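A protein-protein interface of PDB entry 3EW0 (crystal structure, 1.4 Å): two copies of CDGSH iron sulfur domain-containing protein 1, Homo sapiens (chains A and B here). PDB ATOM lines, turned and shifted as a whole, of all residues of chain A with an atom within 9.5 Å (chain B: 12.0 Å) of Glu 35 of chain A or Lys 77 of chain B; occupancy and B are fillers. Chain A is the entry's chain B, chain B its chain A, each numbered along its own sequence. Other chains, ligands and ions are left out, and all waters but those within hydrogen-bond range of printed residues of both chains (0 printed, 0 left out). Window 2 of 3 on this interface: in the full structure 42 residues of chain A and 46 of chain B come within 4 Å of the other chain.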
ATOM      1  N   ALA A  31      22.972 -17.144 -17.997  1.00  0.00           N
ATOM      2  CA  ALA A  31      23.664 -18.335 -18.470  1.00  0.00           C
ATOM      3  C   ALA A  31      22.778 -19.514 -18.181  1.00  0.00           C
ATOM      4  O   ALA A  31      22.344 -19.709 -17.052  1.00  0.00           O
ATOM      5  CB  ALA A  31      25.006 -18.481 -17.790  1.00  0.00           C
ATOM      6  N   PHE A  32      22.498 -20.304 -19.213  1.00  0.00           N
ATOM      7  CA  PHE A  32      21.639 -21.459 -19.069  1.00  0.00           C
ATOM      8  C   PHE A  32      22.378 -22.662 -19.588  1.00  0.00           C
ATOM      9  O   PHE A  32      23.165 -22.568 -20.534  1.00  0.00           O
ATOM     10  CB  PHE A  32      20.345 -21.237 -19.845  1.00  0.00           C
ATOM     11  CG  PHE A  32      19.549 -20.057 -19.364  1.00  0.00           C
ATOM     12  CD1 PHE A  32      18.816 -20.125 -18.195  1.00  0.00           C
ATOM     13  CD2 PHE A  32      19.537 -18.875 -20.068  1.00  0.00           C
ATOM     14  CE1 PHE A  32      18.084 -19.055 -17.742  1.00  0.00           C
ATOM     15  CE2 PHE A  32      18.788 -17.791 -19.631  1.00  0.00           C
ATOM     16  CZ  PHE A  32      18.072 -17.889 -18.457  1.00  0.00           C
ATOM     17  N   ASP A  33      22.127 -23.783 -18.929  1.00  0.00           N
ATOM     18  CA  ASP A  33      22.627 -25.086 -19.344  1.00  0.00           C
ATOM     19  C   ASP A  33      21.726 -25.589 -20.458  1.00  0.00           C
ATOM     20  O   ASP A  33      20.501 -25.629 -20.303  1.00  0.00           O
ATOM     21  CB  ASP A  33      22.615 -26.057 -18.166  1.00  0.00           C
ATOM     22  CG  ASP A  33      23.605 -25.666 -17.087  1.00  0.00           C
ATOM     23  OD1 ASP A  33      24.733 -25.269 -17.434  1.00  0.00           O
ATOM     24  OD2 ASP A  33      23.259 -25.745 -15.889  1.00  0.00           O
ATOM     25  N   MET A  34      22.331 -25.965 -21.583  1.00  0.00           N
ATOM     26  CA  MET A  34      21.567 -26.380 -22.761  1.00  0.00           C
ATOM     27  C   MET A  34      20.757 -27.643 -22.472  1.00  0.00           C
ATOM     28  O   MET A  34      19.637 -27.777 -22.954  1.00  0.00           O
ATOM     29  CB  MET A  34      22.476 -26.571 -23.995  1.00  0.00           C
ATOM     30  CG  MET A  34      23.576 -27.612 -23.878  1.00  0.00           C
ATOM     31  SD  MET A  34      24.697 -27.535 -25.303  1.00  0.00           S
ATOM     32  CE  MET A  34      25.556 -25.986 -25.032  1.00  0.00           C
ATOM     33  N   GLU A  35      21.309 -28.524 -21.644  1.00  0.00           N
ATOM     34  CA  GLU A  35      20.652 -29.785 -21.293  1.00  0.00           C
ATOM     35  C   GLU A  35      19.302 -29.565 -20.607  1.00  0.00           C
ATOM     36  O   GLU A  35      18.397 -30.383 -20.750  1.00  0.00           O
ATOM     37  CB  GLU A  35      21.552 -30.644 -20.392  1.00  0.00           C
ATOM     38  CG  GLU A  35      22.814 -31.179 -21.076  1.00  0.00           C
ATOM     39  CD  GLU A  35      23.974 -30.192 -21.085  1.00  0.00           C
ATOM     40  OE1 GLU A  35      23.768 -29.006 -20.744  1.00  0.00           O
ATOM     41  OE2 GLU A  35      25.098 -30.612 -21.436  1.00  0.00           O
ATOM     42  N   ASP A  36      19.164 -28.456 -19.880  1.00  0.00           N
ATOM     43  CA  ASP A  36      17.940 -28.168 -19.125  1.00  0.00           C
ATOM     44  C   ASP A  36      16.984 -27.197 -19.813  1.00  0.00           C
ATOM     45  O   ASP A  36      16.031 -26.719 -19.190  1.00  0.00           O
ATOM     46  CB  ASP A  36      18.298 -27.646 -17.734  1.00  0.00           C
ATOM     47  CG  ASP A  36      19.037 -28.673 -16.902  1.00  0.00           C
ATOM     48  OD1 ASP A  36      18.818 -29.896 -17.104  1.00  0.00           O
ATOM     49  OD2 ASP A  36      19.830 -28.254 -16.034  1.00  0.00           O
ATOM     50  N   LEU A  37      17.222 -26.905 -21.089  1.00  0.00           N
ATOM     51  CA  LEU A  37      16.253 -26.148 -21.877  1.00  0.00           C
ATOM     52  C   LEU A  37      15.184 -27.142 -22.314  1.00  0.00           C
ATOM     53  O   LEU A  37      15.399 -28.355 -22.262  1.00  0.00           O
ATOM     54  CB  LEU A  37      16.908 -25.486 -23.098  1.00  0.00           C
ATOM     55  CG  LEU A  37      18.105 -24.575 -22.826  1.00  0.00           C
ATOM     56  CD1 LEU A  37      18.752 -24.062 -24.122  1.00  0.00           C
ATOM     57  CD2 LEU A  37      17.661 -23.428 -21.951  1.00  0.00           C
ATOM     58  N   GLY A  38      14.031 -26.634 -22.730  1.00  0.00           N
ATOM     59  CA  GLY A  38      12.993 -27.490 -23.289  1.00  0.00           C
ATOM     60  C   GLY A  38      13.313 -27.763 -24.747  1.00  0.00           C
ATOM     61  O   GLY A  38      14.485 -27.843 -25.129  1.00  0.00           O
ATOM     62  N   ASP A  39      12.279 -27.892 -25.570  1.00  0.00           N
ATOM     63  CA  ASP A  39      12.467 -28.026 -27.011  1.00  0.00           C
ATOM     64  C   ASP A  39      12.876 -26.700 -27.643  1.00  0.00           C
ATOM     65  O   ASP A  39      13.532 -26.677 -28.679  1.00  0.00           O
ATOM     66  CB  ASP A  39      11.191 -28.569 -27.674  1.00  0.00           C
ATOM     67  N   TYR A  43      14.984 -15.815 -26.669  1.00  0.00           N
ATOM     68  CA  TYR A  43      15.616 -14.838 -25.770  1.00  0.00           C
ATOM     69  C   TYR A  43      15.559 -13.437 -26.336  1.00  0.00           C
ATOM     70  O   TYR A  43      15.802 -13.216 -27.511  1.00  0.00           O
ATOM     71  CB  TYR A  43      17.076 -15.242 -25.484  1.00  0.00           C
ATOM     72  CG  TYR A  43      17.212 -16.573 -24.795  1.00  0.00           C
ATOM     73  CD1 TYR A  43      17.003 -16.701 -23.431  1.00  0.00           C
ATOM     74  CD2 TYR A  43      17.488 -17.723 -25.524  1.00  0.00           C
ATOM     75  CE1 TYR A  43      17.117 -17.936 -22.811  1.00  0.00           C
ATOM     76  CE2 TYR A  43      17.604 -18.990 -24.891  1.00  0.00           C
ATOM     77  CZ  TYR A  43      17.407 -19.067 -23.538  1.00  0.00           C
ATOM     78  OH  TYR A  43      17.495 -20.287 -22.914  1.00  0.00           O
ATOM     79  N   ILE A  75      16.944 -20.705 -29.428  1.00  0.00           N
ATOM     80  CA  ILE A  75      17.730 -21.926 -29.236  1.00  0.00           C
ATOM     81  C   ILE A  75      16.765 -23.100 -29.255  1.00  0.00           C
ATOM     82  O   ILE A  75      15.831 -23.142 -28.452  1.00  0.00           O
ATOM     83  CB  ILE A  75      18.504 -21.935 -27.885  1.00  0.00           C
ATOM     84  CG1 ILE A  75      19.487 -20.757 -27.792  1.00  0.00           C
ATOM     85  CG2 ILE A  75      19.222 -23.292 -27.667  1.00  0.00           C
ATOM     86  CD1 ILE A  75      20.610 -20.754 -28.835  1.00  0.00           C
ATOM     87  N   PHE B  32      19.611 -21.209 -33.496  1.00  0.00           N
ATOM     88  CA  PHE B  32      20.638 -22.260 -33.456  1.00  0.00           C
ATOM     89  C   PHE B  32      20.113 -23.569 -32.869  1.00  0.00           C
ATOM     90  O   PHE B  32      19.219 -23.559 -32.028  1.00  0.00           O
ATOM     91  CB  PHE B  32      21.844 -21.780 -32.640  1.00  0.00           C
ATOM     92  CG  PHE B  32      22.524 -20.544 -33.208  1.00  0.00           C
ATOM     93  CD1 PHE B  32      23.471 -20.667 -34.215  1.00  0.00           C
ATOM     94  CD2 PHE B  32      22.232 -19.286 -32.736  1.00  0.00           C
ATOM     95  CE1 PHE B  32      24.117 -19.571 -34.743  1.00  0.00           C
ATOM     96  CE2 PHE B  32      22.879 -18.170 -33.264  1.00  0.00           C
ATOM     97  CZ  PHE B  32      23.818 -18.317 -34.269  1.00  0.00           C
ATOM     98  N   ASP B  33      20.699 -24.692 -33.290  1.00  0.00           N
ATOM     99  CA  ASP B  33      20.383 -25.992 -32.700  1.00  0.00           C
ATOM    100  C   ASP B  33      21.361 -26.284 -31.573  1.00  0.00           C
ATOM    101  O   ASP B  33      22.570 -26.099 -31.738  1.00  0.00           O
ATOM    102  CB  ASP B  33      20.460 -27.103 -33.749  1.00  0.00           C
ATOM    103  CG  ASP B  33      19.386 -26.980 -34.822  1.00  0.00           C
ATOM    104  OD1 ASP B  33      18.260 -26.532 -34.516  1.00  0.00           O
ATOM    105  OD2 ASP B  33      19.668 -27.356 -35.985  1.00  0.00           O
ATOM    106  N   MET B  34      20.832 -26.724 -30.435  1.00  0.00           N
ATOM    107  CA  MET B  34      21.638 -27.094 -29.274  1.00  0.00           C
ATOM    108  C   MET B  34      22.672 -28.153 -29.633  1.00  0.00           C
ATOM    109  O   MET B  34      23.842 -28.046 -29.265  1.00  0.00           O
ATOM    110  CB  MET B  34      20.743 -27.646 -28.156  1.00  0.00           C
ATOM    111  N   GLU B  35      22.227 -29.160 -30.380  1.00  0.00           N
ATOM    112  CA  GLU B  35      23.042 -30.319 -30.723  1.00  0.00           C
ATOM    113  C   GLU B  35      24.326 -29.985 -31.483  1.00  0.00           C
ATOM    114  O   GLU B  35      25.232 -30.822 -31.566  1.00  0.00           O
ATOM    115  CB  GLU B  35      22.219 -31.303 -31.558  1.00  0.00           C
ATOM    116  CG  GLU B  35      21.033 -31.916 -30.818  1.00  0.00           C
ATOM    117  CD  GLU B  35      19.758 -31.084 -30.876  1.00  0.00           C
ATOM    118  OE1 GLU B  35      19.792 -29.926 -31.355  1.00  0.00           O
ATOM    119  OE2 GLU B  35      18.716 -31.605 -30.427  1.00  0.00           O
ATOM    120  N   ASP B  36      24.389 -28.784 -32.049  1.00  0.00           N
ATOM    121  CA  ASP B  36      25.552 -28.329 -32.797  1.00  0.00           C
ATOM    122  C   ASP B  36      26.326 -27.203 -32.085  1.00  0.00           C
ATOM    123  O   ASP B  36      27.205 -26.583 -32.687  1.00  0.00           O
ATOM    124  CB  ASP B  36      25.092 -27.909 -34.198  1.00  0.00           C
ATOM    125  CG  ASP B  36      24.335 -29.032 -34.917  1.00  0.00           C
ATOM    126  OD1 ASP B  36      24.702 -30.212 -34.732  1.00  0.00           O
ATOM    127  OD2 ASP B  36      23.375 -28.736 -35.663  1.00  0.00           O
ATOM    128  N   LEU B  37      26.027 -26.962 -30.804  1.00  0.00           N
ATOM    129  CA  LEU B  37      26.794 -26.009 -29.982  1.00  0.00           C
ATOM    130  C   LEU B  37      28.033 -26.649 -29.353  1.00  0.00           C
ATOM    131  O   LEU B  37      28.106 -27.871 -29.188  1.00  0.00           O
ATOM    132  CB  LEU B  37      25.920 -25.426 -28.863  1.00  0.00           C
ATOM    133  CG  LEU B  37      24.756 -24.539 -29.302  1.00  0.00           C
ATOM    134  CD1 LEU B  37      23.975 -24.033 -28.078  1.00  0.00           C
ATOM    135  CD2 LEU B  37      25.246 -23.369 -30.132  1.00  0.00           C
ATOM    136  N   GLY B  38      29.001 -25.811 -28.992  1.00  0.00           N
ATOM    137  CA  GLY B  38      30.205 -26.272 -28.305  1.00  0.00           C
ATOM    138  C   GLY B  38      30.003 -26.343 -26.802  1.00  0.00           C
ATOM    139  O   GLY B  38      28.917 -26.689 -26.334  1.00  0.00           O
ATOM    140  N   ASP B  39      31.045 -26.016 -26.036  1.00  0.00           N
ATOM    141  CA  ASP B  39      30.916 -25.941 -24.577  1.00  0.00           C
ATOM    142  C   ASP B  39      30.134 -24.712 -24.116  1.00  0.00           C
ATOM    143  O   ASP B  39      29.415 -24.786 -23.129  1.00  0.00           O
ATOM    144  CB  ASP B  39      32.292 -25.944 -23.898  1.00  0.00           C
ATOM    145  CG  ASP B  39      33.046 -27.240 -24.104  1.00  0.00           C
ATOM    146  OD1 ASP B  39      32.482 -28.335 -23.845  1.00  0.00           O
ATOM    147  OD2 ASP B  39      34.228 -27.171 -24.506  1.00  0.00           O
ATOM    148  N   LYS B  40      30.282 -23.598 -24.826  1.00  0.00           N
ATOM    149  CA  LYS B  40      29.703 -22.332 -24.400  1.00  0.00           C
ATOM    150  C   LYS B  40      29.516 -21.476 -25.634  1.00  0.00           C
ATOM    151  O   LYS B  40      30.409 -21.408 -26.471  1.00  0.00           O
ATOM    152  CB  LYS B  40      30.672 -21.664 -23.421  1.00  0.00           C
ATOM    153  CG  LYS B  40      30.257 -20.336 -22.815  1.00  0.00           C
ATOM    154  CD  LYS B  40      31.135 -20.051 -21.590  1.00  0.00           C
ATOM    155  CE  LYS B  40      31.409 -18.574 -21.372  1.00  0.00           C
ATOM    156  NZ  LYS B  40      32.423 -18.378 -20.278  1.00  0.00           N
ATOM    157  N   ALA B  41      28.342 -20.873 -25.778  1.00  0.00           N
ATOM    158  CA  ALA B  41      28.129 -19.865 -26.791  1.00  0.00           C
ATOM    159  C   ALA B  41      27.747 -18.581 -26.076  1.00  0.00           C
ATOM    160  O   ALA B  41      26.871 -18.580 -25.210  1.00  0.00           O
ATOM    161  CB  ALA B  41      27.039 -20.302 -27.754  1.00  0.00           C
ATOM    162  N   VAL B  42      28.421 -17.486 -26.411  1.00  0.00           N
ATOM    163  CA  VAL B  42      28.160 -16.201 -25.762  1.00  0.00           C
ATOM    164  C   VAL B  42      27.590 -15.262 -26.806  1.00  0.00           C
ATOM    165  O   VAL B  42      28.294 -14.826 -27.719  1.00  0.00           O
ATOM    166  CB  VAL B  42      29.435 -15.640 -25.088  1.00  0.00           C
ATOM    167  CG1 VAL B  42      29.135 -14.492 -24.180  1.00  0.00           C
ATOM    168  CG2 VAL B  42      30.113 -16.710 -24.276  1.00  0.00           C
ATOM    169  N   TYR B  43      26.298 -14.987 -26.651  1.00  0.00           N
ATOM    170  CA  TYR B  43      25.530 -14.245 -27.628  1.00  0.00           C
ATOM    171  C   TYR B  43      25.378 -12.781 -27.199  1.00  0.00           C
ATOM    172  O   TYR B  43      25.112 -12.467 -26.037  1.00  0.00           O
ATOM    173  CB  TYR B  43      24.162 -14.877 -27.773  1.00  0.00           C
ATOM    174  CG  TYR B  43      24.196 -16.288 -28.293  1.00  0.00           C
ATOM    175  CD1 TYR B  43      24.554 -16.547 -29.608  1.00  0.00           C
ATOM    176  CD2 TYR B  43      23.881 -17.365 -27.475  1.00  0.00           C
ATOM    177  CE1 TYR B  43      24.607 -17.849 -30.079  1.00  0.00           C
ATOM    178  CE2 TYR B  43      23.906 -18.662 -27.941  1.00  0.00           C
ATOM    179  CZ  TYR B  43      24.265 -18.896 -29.246  1.00  0.00           C
ATOM    180  OH  TYR B  43      24.292 -20.205 -29.708  1.00  0.00           O
ATOM    181  N   LEU B  73      24.075 -13.264 -23.364  1.00  0.00           N
ATOM    182  CA  LEU B  73      23.352 -14.454 -22.988  1.00  0.00           C
ATOM    183  C   LEU B  73      24.301 -15.609 -23.291  1.00  0.00           C
ATOM    184  O   LEU B  73      24.874 -15.695 -24.384  1.00  0.00           O
ATOM    185  CB  LEU B  73      22.059 -14.583 -23.802  1.00  0.00           C
ATOM    186  CG  LEU B  73      21.415 -15.973 -23.720  1.00  0.00           C
ATOM    187  CD1 LEU B  73      20.610 -16.115 -22.437  1.00  0.00           C
ATOM    188  CD2 LEU B  73      20.571 -16.247 -24.947  1.00  0.00           C
ATOM    189  N   ILE B  74      24.423 -16.510 -22.318  1.00  0.00           N
ATOM    190  CA  ILE B  74      25.305 -17.645 -22.409  1.00  0.00           C
ATOM    191  C   ILE B  74      24.496 -18.930 -22.419  1.00  0.00           C
ATOM    192  O   ILE B  74      23.628 -19.154 -21.565  1.00  0.00           O
ATOM    193  CB  ILE B  74      26.271 -17.648 -21.223  1.00  0.00           C
ATOM    194  CG1 ILE B  74      27.234 -16.457 -21.298  1.00  0.00           C
ATOM    195  CG2 ILE B  74      27.084 -18.918 -21.193  1.00  0.00           C
ATOM    196  CD1 ILE B  74      28.019 -16.171 -20.035  1.00  0.00           C
ATOM    197  N   ILE B  75      24.776 -19.768 -23.416  1.00  0.00           N
ATOM    198  CA  ILE B  75      24.216 -21.099 -23.465  1.00  0.00           C
ATOM    199  C   ILE B  75      25.418 -22.007 -23.371  1.00  0.00           C
ATOM    200  O   ILE B  75      26.320 -21.904 -24.199  1.00  0.00           O
ATOM    201  CB  ILE B  75      23.429 -21.348 -24.764  1.00  0.00           C
ATOM    202  CG1 ILE B  75      22.271 -20.353 -24.870  1.00  0.00           C
ATOM    203  CG2 ILE B  75      22.938 -22.807 -24.814  1.00  0.00           C
ATOM    204  CD1 ILE B  75      21.275 -20.423 -23.716  1.00  0.00           C
ATOM    205  N   LYS B  76      25.444 -22.846 -22.343  1.00  0.00           N
ATOM    206  CA  LYS B  76      26.607 -23.679 -22.054  1.00  0.00           C
ATOM    207  C   LYS B  76      26.240 -25.130 -21.768  1.00  0.00           C
ATOM    208  O   LYS B  76      25.077 -25.453 -21.520  1.00  0.00           O
ATOM    209  CB  LYS B  76      27.409 -23.101 -20.880  1.00  0.00           C
ATOM    210  CG  LYS B  76      26.646 -23.019 -19.554  1.00  0.00           C
ATOM    211  CD  LYS B  76      27.371 -22.103 -18.566  1.00  0.00           C
ATOM    212  CE  LYS B  76      26.743 -22.146 -17.175  1.00  0.00           C
ATOM    213  NZ  LYS B  76      26.668 -23.502 -16.609  1.00  0.00           N
ATOM    214  N   LYS B  77      27.247 -25.997 -21.805  1.00  0.00           N
ATOM    215  CA  LYS B  77      27.106 -27.374 -21.345  1.00  0.00           C
ATOM    216  C   LYS B  77      27.193 -27.419 -19.824  1.00  0.00           C
ATOM    217  O   LYS B  77      28.102 -26.837 -19.236  1.00  0.00           O
ATOM    218  CB  LYS B  77      28.221 -28.226 -21.930  1.00  0.00           C
ATOM    219  CG  LYS B  77      28.154 -28.384 -23.434  1.00  0.00           C
ATOM    220  CD  LYS B  77      27.070 -29.375 -23.832  1.00  0.00           C
ATOM    221  CE  LYS B  77      27.427 -30.141 -25.114  1.00  0.00           C
ATOM    222  NZ  LYS B  77      28.012 -29.298 -26.195  1.00  0.00           N
ATOM    223  N   LYS B  78      26.237 -28.084 -19.190  1.00  0.00           N
ATOM    224  CA  LYS B  78      26.256 -28.290 -17.738  1.00  0.00           C
ATOM    225  C   LYS B  78      27.528 -29.002 -17.252  1.00  0.00           C
ATOM    226  O   LYS B  78      28.018 -29.932 -17.900  1.00  0.00           O
ATOM    227  CB  LYS B  78      25.011 -29.079 -17.309  1.00  0.00           C
ATOM    228  CG  LYS B  78      24.998 -29.512 -15.842  1.00  0.00           C
ATOM    229  CD  LYS B  78      23.586 -29.829 -15.352  1.00  0.00           C
ATOM    230  CE  LYS B  78      22.745 -28.565 -15.223  1.00  0.00           C
ATOM    231  N   GLU B  79      28.042 -28.555 -16.103  1.00  0.00           N
ATOM    232  CA  GLU B  79      29.242 -29.129 -15.475  1.00  0.00           C
ATOM    233  C   GLU B  79      29.452 -30.614 -15.794  1.00  0.00           C
ATOM    234  O   GLU B  79      29.310 -31.491 -14.941  1.00  0.00           O
ATOM    235  CB  GLU B  79      29.181 -28.930 -13.954  1.00  0.00           C
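The backbone carbonyl oxygen (O) of Ile 74 of chain B is in hydrogen-bond range of the backbone NH (N) of Phe 32 of chain A.
The backbone NH (N) of Met 34 of chain A lies within hydrogen-bond range of the backbone carbonyl oxygen (O) of Lys 76 of chain B, 2.8 Å away.
The backbone NH of Lys 76 of chain B lies within hydrogen-bond range of the backbone carbonyl oxygen of Phe 32 of chain A, 2.9 Å away.
NZ of Lys 76 of chain B is in salt-bridge range of OD1 of Asp 33 of chain A (2.7 Å).
The backbone NH of Lys 78 of chain B is in hydrogen-bond range of the side-chain carboxylate of Glu 35 of chain A.
The backbone carbonyl oxygen (O) of Leu 73 of chain B lies within hydrogen-bond range of the backbone NH (N) of Tyr 43 of chain B, 2.8 Å away.
The side-chain amino group (NZ) of Lys 77 of chain B is in hydrogen-bond range of the backbone carbonyl oxygen (O) of Gly 38 of chain B (2.8 Å).
The backbone NH (N) of Lys 77 of chain B sits at hydrogen-bond distance from the backbone carbonyl oxygen (O) of Asp 39 of chain B, at 2.8 Å.
N of Ala 41 of chain B sits at hydrogen-bond distance from O of Ile 75 of chain B, at 2.8 Å.
The side-chain amino group of Lys 77 of chain B lies within hydrogen-bond range of the backbone carbonyl oxygen of Leu 37 of chain B (3.3 Å).
Ala 31 of chain A touches Ile 74 of chain B.
Phe 32 of chain A touches Leu 73 of chain B (CE2 to CD1, 3.7 Å).
Asp 33 of chain A touches Lys 78 of chain B (OD2 to CE, 2.9 Å).
Met 34 of chain A touches Gly 38 of chain B.
Met 34 of chain A touches Ile 75 of chain B (CB to CG2, 3.9 Å).
Met 34 of chain A touches Lys 77 of chain B.
O of Lys 76 of chain B touches OE1 of Glu 35 of chain A, 3.9 Å away.
OE2 of Glu 35 of chain A touches CD of Lys 77 of chain B (3.3 Å).
OH of Tyr 43 of chain A touches CD1 of Ile 75 of chain B (3.9 Å).
CA of Ile 75 of chain A touches O of Phe 32 of chain B (3.6 Å).
Glu 35 of chain A touches just these residues of chain B: Lys 76, Lys 77 and Lys 78.
Asp 33 of chain A touches two residues of chain B.
Leu 37 of chain A touches none of the printed residues of chain B.
No residue of chain B comes within 4 Å of Gly 38 of chain A.
Of chain A, only Met 34 comes within 4 Å of Gly 38 of chain B.
Lys 76 of chain B touches just these residues of chain A: Phe 32 (2.9 Å), Asp 33 (2.7 Å), Met 34 (2.8 Å) and Glu 35 (3.9 Å).
Of the printed residues of chain A, Phe 32 of chain B touches Ile 75.
Printed residues of chain B within 4 Å of Phe 32 of chain A: Leu 73 (3.7 Å), Ile 74 (2.9 Å), Ile 75 (3.4 Å) and Lys 76 (2.9 Å).
Printed residues of chain B within 4 Å of Ile 75 of chain A: Phe 32 and Tyr 43.
Of the printed residues of chain A, Ile 74 of chain B touches Ala 31 and Phe 32.
Of the printed residues of chain B, Ala 31 of chain A touches Ile 74 (3.2 Å).
The nearest residue of chain A that does not touch Lys 77 of chain B is Asp 33 of chain A (4.05 Å).
Of the 11 printed residues of chain A, 8 touch a printed residue of chain B.
Hydrophobic or aromatic side chains of chain A that line the printed part of chain B: Ala 31, Phe 32, Met 34, Tyr 43 and Ile 75.
Along chain A the printed residues that touch a printed residue of chain B span positions 31 to 75.
Phe 32 of chain A touches Ile 75 of chain B, and with the chains exchanged Ile 75 of chain A touches Phe 32 of chain B.
Met 34 of chain A touches Leu 37 of chain B, but with the chains exchanged Leu 37 of chain A does not touch Met 34 of chain B (5.8 Å).
Met 34 of chain A touches Ile 75 of chain B, but with the chains exchanged Ile 75 of chain A does not touch Met 34 of chain B (4.6 Å).
Tyr 43 of chain A touches Ile 75 of chain B, and with the chains exchanged Ile 75 of chain A touches Tyr 43 of chain B.
Positions printed for both chains: 32, 33, 34, 35, 36, 37, 38, 39, 43 and 75.
Of the 20 pairs that touch across the chains among the printed residues, 4 have their exchanged pair printed and touching as well.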
